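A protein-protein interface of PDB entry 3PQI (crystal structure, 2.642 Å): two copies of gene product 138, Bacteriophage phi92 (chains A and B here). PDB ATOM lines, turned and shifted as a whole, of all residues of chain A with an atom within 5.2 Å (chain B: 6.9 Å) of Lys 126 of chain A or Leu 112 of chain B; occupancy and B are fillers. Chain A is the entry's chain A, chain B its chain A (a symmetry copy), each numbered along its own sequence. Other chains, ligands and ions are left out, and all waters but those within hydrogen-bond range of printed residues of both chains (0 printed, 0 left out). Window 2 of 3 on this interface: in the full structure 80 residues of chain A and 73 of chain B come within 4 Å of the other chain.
Of the 15 printed residues of chain B, 5 touch a printed residue of chain A.
Hydrophobic or aromatic side chains of chain B that line the printed part of chain A: Leu 112, Ile 113 and Leu 118.
Among the printed residues, 10 pairs touch across the chains.
Among the printed residues, no Asp or Glu carboxylate lies within 4 Å of a Lys or Arg side-chain nitrogen of the other chain.
Of the printed residues of chain B, Ile 124 of chain A touches Leu 112 (3.6 Å), Ile 113 (3.8 Å) and Leu 118 (3.97 Å).
Lys 126 of chain A touches just these residues of chain B: Thr 111 (3.5 Å) and Leu 112 (3.97 Å).
Of the printed residues of chain B, Ile 127 of chain A touches Gly 110, Thr 111 and Ile 113.
Of the printed residues of chain A, Gly 110 of chain B touches Ile 127.
Of the printed residues of chain A, Thr 111 of chain B touches Lys 126 (3.5 Å) and Ile 127 (2.9 Å).
Leu 112 of chain B touches just these residues of chain A: Ile 124, Pro 125 and Lys 126.
The nearest residue of chain A that does not touch Leu 112 of chain B is Val 88 of chain A (4.4 Å).
The nearest printed residue of chain A that does not touch Leu 118 of chain B is Val 88 of chain A (5.7 Å).
Among the printed residues, pairs that only touch across the chains: Lys 126 of chain A with Thr 111 of chain B, Pro 125 of chain A with Ile 113 of chain B, Ile 124 of chain A with Leu 112 of chain B, Pro 125 of chain A with Leu 112 of chain B, Ile 124 of chain A with Ile 113 of chain B, Ile 127 of chain A with Gly 110 of chain B, Ile 127 of chain A with Ile 113 of chain B, Ile 124 of chain A with Leu 118 of chain B and Lys 126 of chain A with Leu 112 of chain B.
The backbone carbonyl oxygen of Ile 86 of chain A lies within hydrogen-bond range of the backbone NH of Lys 126 of chain A (3.1 Å).
The backbone NH of Val 88 of chain A is in hydrogen-bond range of the backbone carbonyl oxygen of Ile 124 of chain A (2.8 Å).
N of Val 69 of chain B is in hydrogen-bond range of O of Ile 113 of chain B, 3.0 Å away.
The backbone carbonyl oxygen of Ile 127 of chain A lies within hydrogen-bond range of the backbone NH of Thr 111 of chain B, 2.9 Å away.
No position is printed for both chains.
Of the 10 pairs that touch across the chains among the printed residues, none has its exchanged pair printed and touching as well.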
ATOM      1  N   ILE A  86      -5.959  20.852 -21.228  1.00  0.00           N
ATOM      2  CA  ILE A  86      -6.693  19.658 -21.615  1.00  0.00           C
ATOM      3  C   ILE A  86      -7.278  18.963 -20.384  1.00  0.00           C
ATOM      4  O   ILE A  86      -6.754  19.079 -19.269  1.00  0.00           O
ATOM      5  CB  ILE A  86      -5.777  18.675 -22.383  1.00  0.00           C
ATOM      6  CG1 ILE A  86      -5.296  19.309 -23.690  1.00  0.00           C
ATOM      7  CG2 ILE A  86      -6.492  17.357 -22.662  1.00  0.00           C
ATOM      8  CD1 ILE A  86      -6.415  19.680 -24.637  1.00  0.00           C
ATOM      9  N   GLY A  87      -8.373  18.245 -20.588  1.00  0.00           N
ATOM     10  CA  GLY A  87      -9.008  17.516 -19.510  1.00  0.00           C
ATOM     11  C   GLY A  87     -10.152  16.677 -20.032  1.00  0.00           C
ATOM     12  O   GLY A  87     -10.175  16.296 -21.202  1.00  0.00           O
ATOM     13  N   VAL A  88     -11.111  16.393 -19.161  1.00  0.00           N
ATOM     14  CA  VAL A  88     -12.258  15.587 -19.544  1.00  0.00           C
ATOM     15  C   VAL A  88     -13.525  16.078 -18.864  1.00  0.00           C
ATOM     16  O   VAL A  88     -13.551  16.282 -17.653  1.00  0.00           O
ATOM     17  CB  VAL A  88     -12.044  14.098 -19.194  1.00  0.00           C
ATOM     18  CG1 VAL A  88     -13.358  13.341 -19.269  1.00  0.00           C
ATOM     19  CG2 VAL A  88     -11.006  13.475 -20.117  1.00  0.00           C
ATOM     20  N   ILE A 124     -12.596  17.934 -15.427  1.00  0.00           N
ATOM     21  CA  ILE A 124     -11.483  17.326 -14.718  1.00  0.00           C
ATOM     22  C   ILE A 124     -10.200  17.481 -15.526  1.00  0.00           C
ATOM     23  O   ILE A 124     -10.070  16.909 -16.608  1.00  0.00           O
ATOM     24  CB  ILE A 124     -11.739  15.835 -14.449  1.00  0.00           C
ATOM     25  CG1 ILE A 124     -13.111  15.640 -13.800  1.00  0.00           C
ATOM     26  CG2 ILE A 124     -10.637  15.253 -13.570  1.00  0.00           C
ATOM     27  CD1 ILE A 124     -13.477  14.184 -13.572  1.00  0.00           C
ATOM     28  N   PRO A 125      -9.247  18.268 -15.002  1.00  0.00           N
ATOM     29  CA  PRO A 125      -7.961  18.474 -15.675  1.00  0.00           C
ATOM     30  C   PRO A 125      -7.194  17.165 -15.831  1.00  0.00           C
ATOM     31  O   PRO A 125      -7.148  16.349 -14.908  1.00  0.00           O
ATOM     32  CB  PRO A 125      -7.212  19.414 -14.723  1.00  0.00           C
ATOM     33  CG  PRO A 125      -8.280  20.070 -13.919  1.00  0.00           C
ATOM     34  CD  PRO A 125      -9.337  19.031 -13.746  1.00  0.00           C
ATOM     35  N   LYS A 126      -6.608  16.965 -17.004  1.00  0.00           N
ATOM     36  CA  LYS A 126      -5.770  15.801 -17.244  1.00  0.00           C
ATOM     37  C   LYS A 126      -4.326  16.267 -17.376  1.00  0.00           C
ATOM     38  O   LYS A 126      -3.793  16.377 -18.481  1.00  0.00           O
ATOM     39  CB  LYS A 126      -6.225  15.055 -18.500  1.00  0.00           C
ATOM     40  CG  LYS A 126      -5.617  13.673 -18.651  1.00  0.00           C
ATOM     41  CD  LYS A 126      -6.218  12.940 -19.839  1.00  0.00           C
ATOM     42  CE  LYS A 126      -5.568  11.580 -20.043  1.00  0.00           C
ATOM     43  NZ  LYS A 126      -6.100  10.894 -21.252  1.00  0.00           N
ATOM     44  N   ILE A 127      -3.705  16.548 -16.233  1.00  0.00           N
ATOM     45  CA  ILE A 127      -2.361  17.117 -16.190  1.00  0.00           C
ATOM     46  C   ILE A 127      -1.273  16.072 -16.442  1.00  0.00           C
ATOM     47  O   ILE A 127      -1.454  14.889 -16.158  1.00  0.00           O
ATOM     48  CB  ILE A 127      -2.098  17.814 -14.841  1.00  0.00           C
ATOM     49  CG1 ILE A 127      -1.955  16.777 -13.725  1.00  0.00           C
ATOM     50  CG2 ILE A 127      -3.214  18.808 -14.527  1.00  0.00           C
ATOM     51  CD1 ILE A 127      -1.866  17.381 -12.338  1.00  0.00           C
ATOM     52  N   ALA A 128      -0.144  16.521 -16.984  1.00  0.00           N
ATOM     53  CA  ALA A 128       0.972  15.631 -17.283  1.00  0.00           C
ATOM     54  C   ALA A 128       1.828  15.391 -16.045  1.00  0.00           C
ATOM     55  O   ALA A 128       2.158  16.328 -15.312  1.00  0.00           O
ATOM     56  CB  ALA A 128       1.819  16.198 -18.417  1.00  0.00           C
ATOM     57  N   LYS B  39       1.586   7.724 -11.400  1.00  0.00           N
ATOM     58  CA  LYS B  39       0.621   7.966 -10.331  1.00  0.00           C
ATOM     59  C   LYS B  39      -0.206   6.706 -10.116  1.00  0.00           C
ATOM     60  O   LYS B  39      -1.434   6.750 -10.089  1.00  0.00           O
ATOM     61  CB  LYS B  39      -0.292   9.149 -10.665  1.00  0.00           C
ATOM     62  CG  LYS B  39       0.452  10.444 -10.951  1.00  0.00           C
ATOM     63  CD  LYS B  39       1.304  10.864  -9.764  1.00  0.00           C
ATOM     64  CE  LYS B  39       2.269  11.975 -10.144  1.00  0.00           C
ATOM     65  NZ  LYS B  39       3.222  11.540 -11.207  1.00  0.00           N
ATOM     66  N   PRO B  66      -4.583   3.549 -10.009  1.00  0.00           N
ATOM     67  CA  PRO B  66      -4.312   4.979  -9.835  1.00  0.00           C
ATOM     68  C   PRO B  66      -4.898   5.562  -8.555  1.00  0.00           C
ATOM     69  O   PRO B  66      -5.671   4.905  -7.858  1.00  0.00           O
ATOM     70  CB  PRO B  66      -5.019   5.597 -11.039  1.00  0.00           C
ATOM     71  CG  PRO B  66      -6.197   4.709 -11.246  1.00  0.00           C
ATOM     72  CD  PRO B  66      -5.729   3.313 -10.905  1.00  0.00           C
ATOM     73  N   PHE B  67      -4.529   6.806  -8.266  1.00  0.00           N
ATOM     74  CA  PHE B  67      -5.043   7.522  -7.107  1.00  0.00           C
ATOM     75  C   PHE B  67      -5.237   9.004  -7.424  1.00  0.00           C
ATOM     76  O   PHE B  67      -4.663   9.521  -8.383  1.00  0.00           O
ATOM     77  CB  PHE B  67      -4.103   7.350  -5.910  1.00  0.00           C
ATOM     78  CG  PHE B  67      -2.650   7.601  -6.228  1.00  0.00           C
ATOM     79  CD1 PHE B  67      -2.143   8.892  -6.262  1.00  0.00           C
ATOM     80  CD2 PHE B  67      -1.788   6.542  -6.473  1.00  0.00           C
ATOM     81  CE1 PHE B  67      -0.805   9.122  -6.547  1.00  0.00           C
ATOM     82  CE2 PHE B  67      -0.450   6.766  -6.755  1.00  0.00           C
ATOM     83  CZ  PHE B  67       0.042   8.056  -6.792  1.00  0.00           C
ATOM     84  N   MET B  68      -6.049   9.678  -6.615  1.00  0.00           N
ATOM     85  CA  MET B  68      -6.299  11.105  -6.794  1.00  0.00           C
ATOM     86  C   MET B  68      -5.063  11.950  -6.491  1.00  0.00           C
ATOM     87  O   MET B  68      -4.401  11.760  -5.470  1.00  0.00           O
ATOM     88  CB  MET B  68      -7.456  11.568  -5.903  1.00  0.00           C
ATOM     89  CG  MET B  68      -7.520  13.085  -5.740  1.00  0.00           C
ATOM     90  SD  MET B  68      -8.664  13.665  -4.473  1.00  0.00           S
ATOM     91  CE  MET B  68      -8.285  15.415  -4.478  1.00  0.00           C
ATOM     92  N   VAL B  69      -4.761  12.890  -7.381  1.00  0.00           N
ATOM     93  CA  VAL B  69      -3.720  13.879  -7.118  1.00  0.00           C
ATOM     94  C   VAL B  69      -4.310  15.283  -7.168  1.00  0.00           C
ATOM     95  O   VAL B  69      -5.302  15.524  -7.853  1.00  0.00           O
ATOM     96  CB  VAL B  69      -2.550  13.770  -8.116  1.00  0.00           C
ATOM     97  CG1 VAL B  69      -1.779  12.476  -7.887  1.00  0.00           C
ATOM     98  CG2 VAL B  69      -3.056  13.857  -9.546  1.00  0.00           C
ATOM     99  N   SER B 109      -0.083   7.290 -21.575  1.00  0.00           N
ATOM    100  CA  SER B 109       0.265   8.372 -20.657  1.00  0.00           C
ATOM    101  C   SER B 109      -0.973   9.105 -20.131  1.00  0.00           C
ATOM    102  O   SER B 109      -1.913   9.373 -20.882  1.00  0.00           O
ATOM    103  CB  SER B 109       1.217   9.362 -21.335  1.00  0.00           C
ATOM    104  OG  SER B 109       2.427   8.731 -21.726  1.00  0.00           O
ATOM    105  N   GLY B 110      -0.962   9.426 -18.839  1.00  0.00           N
ATOM    106  CA  GLY B 110      -2.070  10.118 -18.202  1.00  0.00           C
ATOM    107  C   GLY B 110      -1.838  11.616 -18.110  1.00  0.00           C
ATOM    108  O   GLY B 110      -1.251  12.212 -19.015  1.00  0.00           O
ATOM    109  N   THR B 111      -2.297  12.228 -17.021  1.00  0.00           N
ATOM    110  CA  THR B 111      -3.008  11.516 -15.962  1.00  0.00           C
ATOM    111  C   THR B 111      -4.138  12.369 -15.368  1.00  0.00           C
ATOM    112  O   THR B 111      -4.001  13.582 -15.205  1.00  0.00           O
ATOM    113  CB  THR B 111      -2.051  11.073 -14.828  1.00  0.00           C
ATOM    114  OG1 THR B 111      -2.704  10.111 -13.993  1.00  0.00           O
ATOM    115  CG2 THR B 111      -1.623  12.267 -13.984  1.00  0.00           C
ATOM    116  N   LEU B 112      -5.251  11.717 -15.045  1.00  0.00           N
ATOM    117  CA  LEU B 112      -6.424  12.402 -14.509  1.00  0.00           C
ATOM    118  C   LEU B 112      -6.309  12.599 -12.995  1.00  0.00           C
ATOM    119  O   LEU B 112      -5.892  11.690 -12.276  1.00  0.00           O
ATOM    120  CB  LEU B 112      -7.689  11.609 -14.848  1.00  0.00           C
ATOM    121  CG  LEU B 112      -9.005  12.379 -14.985  1.00  0.00           C
ATOM    122  CD1 LEU B 112      -8.937  13.376 -16.137  1.00  0.00           C
ATOM    123  CD2 LEU B 112     -10.160  11.411 -15.181  1.00  0.00           C
ATOM    124  N   ILE B 113      -6.685  13.783 -12.513  1.00  0.00           N
ATOM    125  CA  ILE B 113      -6.528  14.112 -11.094  1.00  0.00           C
ATOM    126  C   ILE B 113      -7.548  13.424 -10.181  1.00  0.00           C
ATOM    127  O   ILE B 113      -7.232  13.088  -9.042  1.00  0.00           O
ATOM    128  CB  ILE B 113      -6.538  15.643 -10.842  1.00  0.00           C
ATOM    129  CG1 ILE B 113      -7.940  16.225 -11.053  1.00  0.00           C
ATOM    130  CG2 ILE B 113      -5.503  16.333 -11.727  1.00  0.00           C
ATOM    131  CD1 ILE B 113      -8.104  17.639 -10.530  1.00  0.00           C
ATOM    132  N   GLN B 114      -8.766  13.223 -10.674  1.00  0.00           N
ATOM    133  CA  GLN B 114      -9.779  12.475  -9.929  1.00  0.00           C
ATOM    134  C   GLN B 114     -10.280  11.289 -10.755  1.00  0.00           C
ATOM    135  O   GLN B 114     -11.183  11.436 -11.582  1.00  0.00           O
ATOM    136  CB  GLN B 114     -10.943  13.381  -9.518  1.00  0.00           C
ATOM    137  CG  GLN B 114     -11.289  13.326  -8.026  1.00  0.00           C
ATOM    138  CD  GLN B 114     -11.832  11.975  -7.581  1.00  0.00           C
ATOM    139  OE1 GLN B 114     -10.981  10.952  -7.602  1.00  0.00           O
ATOM    140  NE2 GLN B 114     -13.003  11.857  -7.216  1.00  0.00           N
ATOM    141  N   PRO B 115      -9.691  10.106 -10.524  1.00  0.00           N
ATOM    142  CA  PRO B 115      -9.940   8.916 -11.339  1.00  0.00           C
ATOM    143  C   PRO B 115     -11.040   8.011 -10.785  1.00  0.00           C
ATOM    144  O   PRO B 115     -11.456   7.074 -11.468  1.00  0.00           O
ATOM    145  CB  PRO B 115      -8.590   8.191 -11.295  1.00  0.00           C
ATOM    146  CG  PRO B 115      -7.927   8.666  -9.997  1.00  0.00           C
ATOM    147  CD  PRO B 115      -8.732   9.819  -9.444  1.00  0.00           C
ATOM    148  N   CYS B 116     -11.501   8.286  -9.567  1.00  0.00           N
ATOM    149  CA  CYS B 116     -12.524   7.457  -8.940  1.00  0.00           C
ATOM    150  C   CYS B 116     -13.882   7.614  -9.611  1.00  0.00           C
ATOM    151  O   CYS B 116     -14.278   8.718  -9.993  1.00  0.00           O
ATOM    152  CB  CYS B 116     -12.624   7.758  -7.445  1.00  0.00           C
ATOM    153  SG  CYS B 116     -11.205   7.172  -6.494  1.00  0.00           S
ATOM    154  N   LEU B 118     -14.706   6.716 -12.495  1.00  0.00           N
ATOM    155  CA  LEU B 118     -14.535   6.611 -13.943  1.00  0.00           C
ATOM    156  C   LEU B 118     -13.405   5.658 -14.354  1.00  0.00           C
ATOM    157  O   LEU B 118     -13.193   5.406 -15.541  1.00  0.00           O
ATOM    158  CB  LEU B 118     -14.352   7.999 -14.570  1.00  0.00           C
ATOM    159  CG  LEU B 118     -13.173   8.865 -14.123  1.00  0.00           C
ATOM    160  CD1 LEU B 118     -11.893   8.388 -14.778  1.00  0.00           C
ATOM    161  CD2 LEU B 118     -13.429  10.321 -14.472  1.00  0.00           C
ATOM    162  N   TYR B 119     -12.682   5.143 -13.366  1.00  0.00           N
ATOM    163  CA  TYR B 119     -11.720   4.070 -13.594  1.00  0.00           C
ATOM    164  C   TYR B 119     -12.278   2.778 -13.009  1.00  0.00           C
ATOM    165  O   TYR B 119     -13.060   2.814 -12.058  1.00  0.00           O
ATOM    166  CB  TYR B 119     -10.366   4.395 -12.956  1.00  0.00           C
ATOM    167  CG  TYR B 119      -9.396   5.091 -13.883  1.00  0.00           C
ATOM    168  CD1 TYR B 119      -8.447   4.369 -14.597  1.00  0.00           C
ATOM    169  CD2 TYR B 119      -9.429   6.469 -14.044  1.00  0.00           C
ATOM    170  CE1 TYR B 119      -7.558   5.005 -15.449  1.00  0.00           C
ATOM    171  CE2 TYR B 119      -8.549   7.113 -14.893  1.00  0.00           C
ATOM    172  CZ  TYR B 119      -7.616   6.379 -15.592  1.00  0.00           C
ATOM    173  OH  TYR B 119      -6.739   7.025 -16.436  1.00  0.00           O
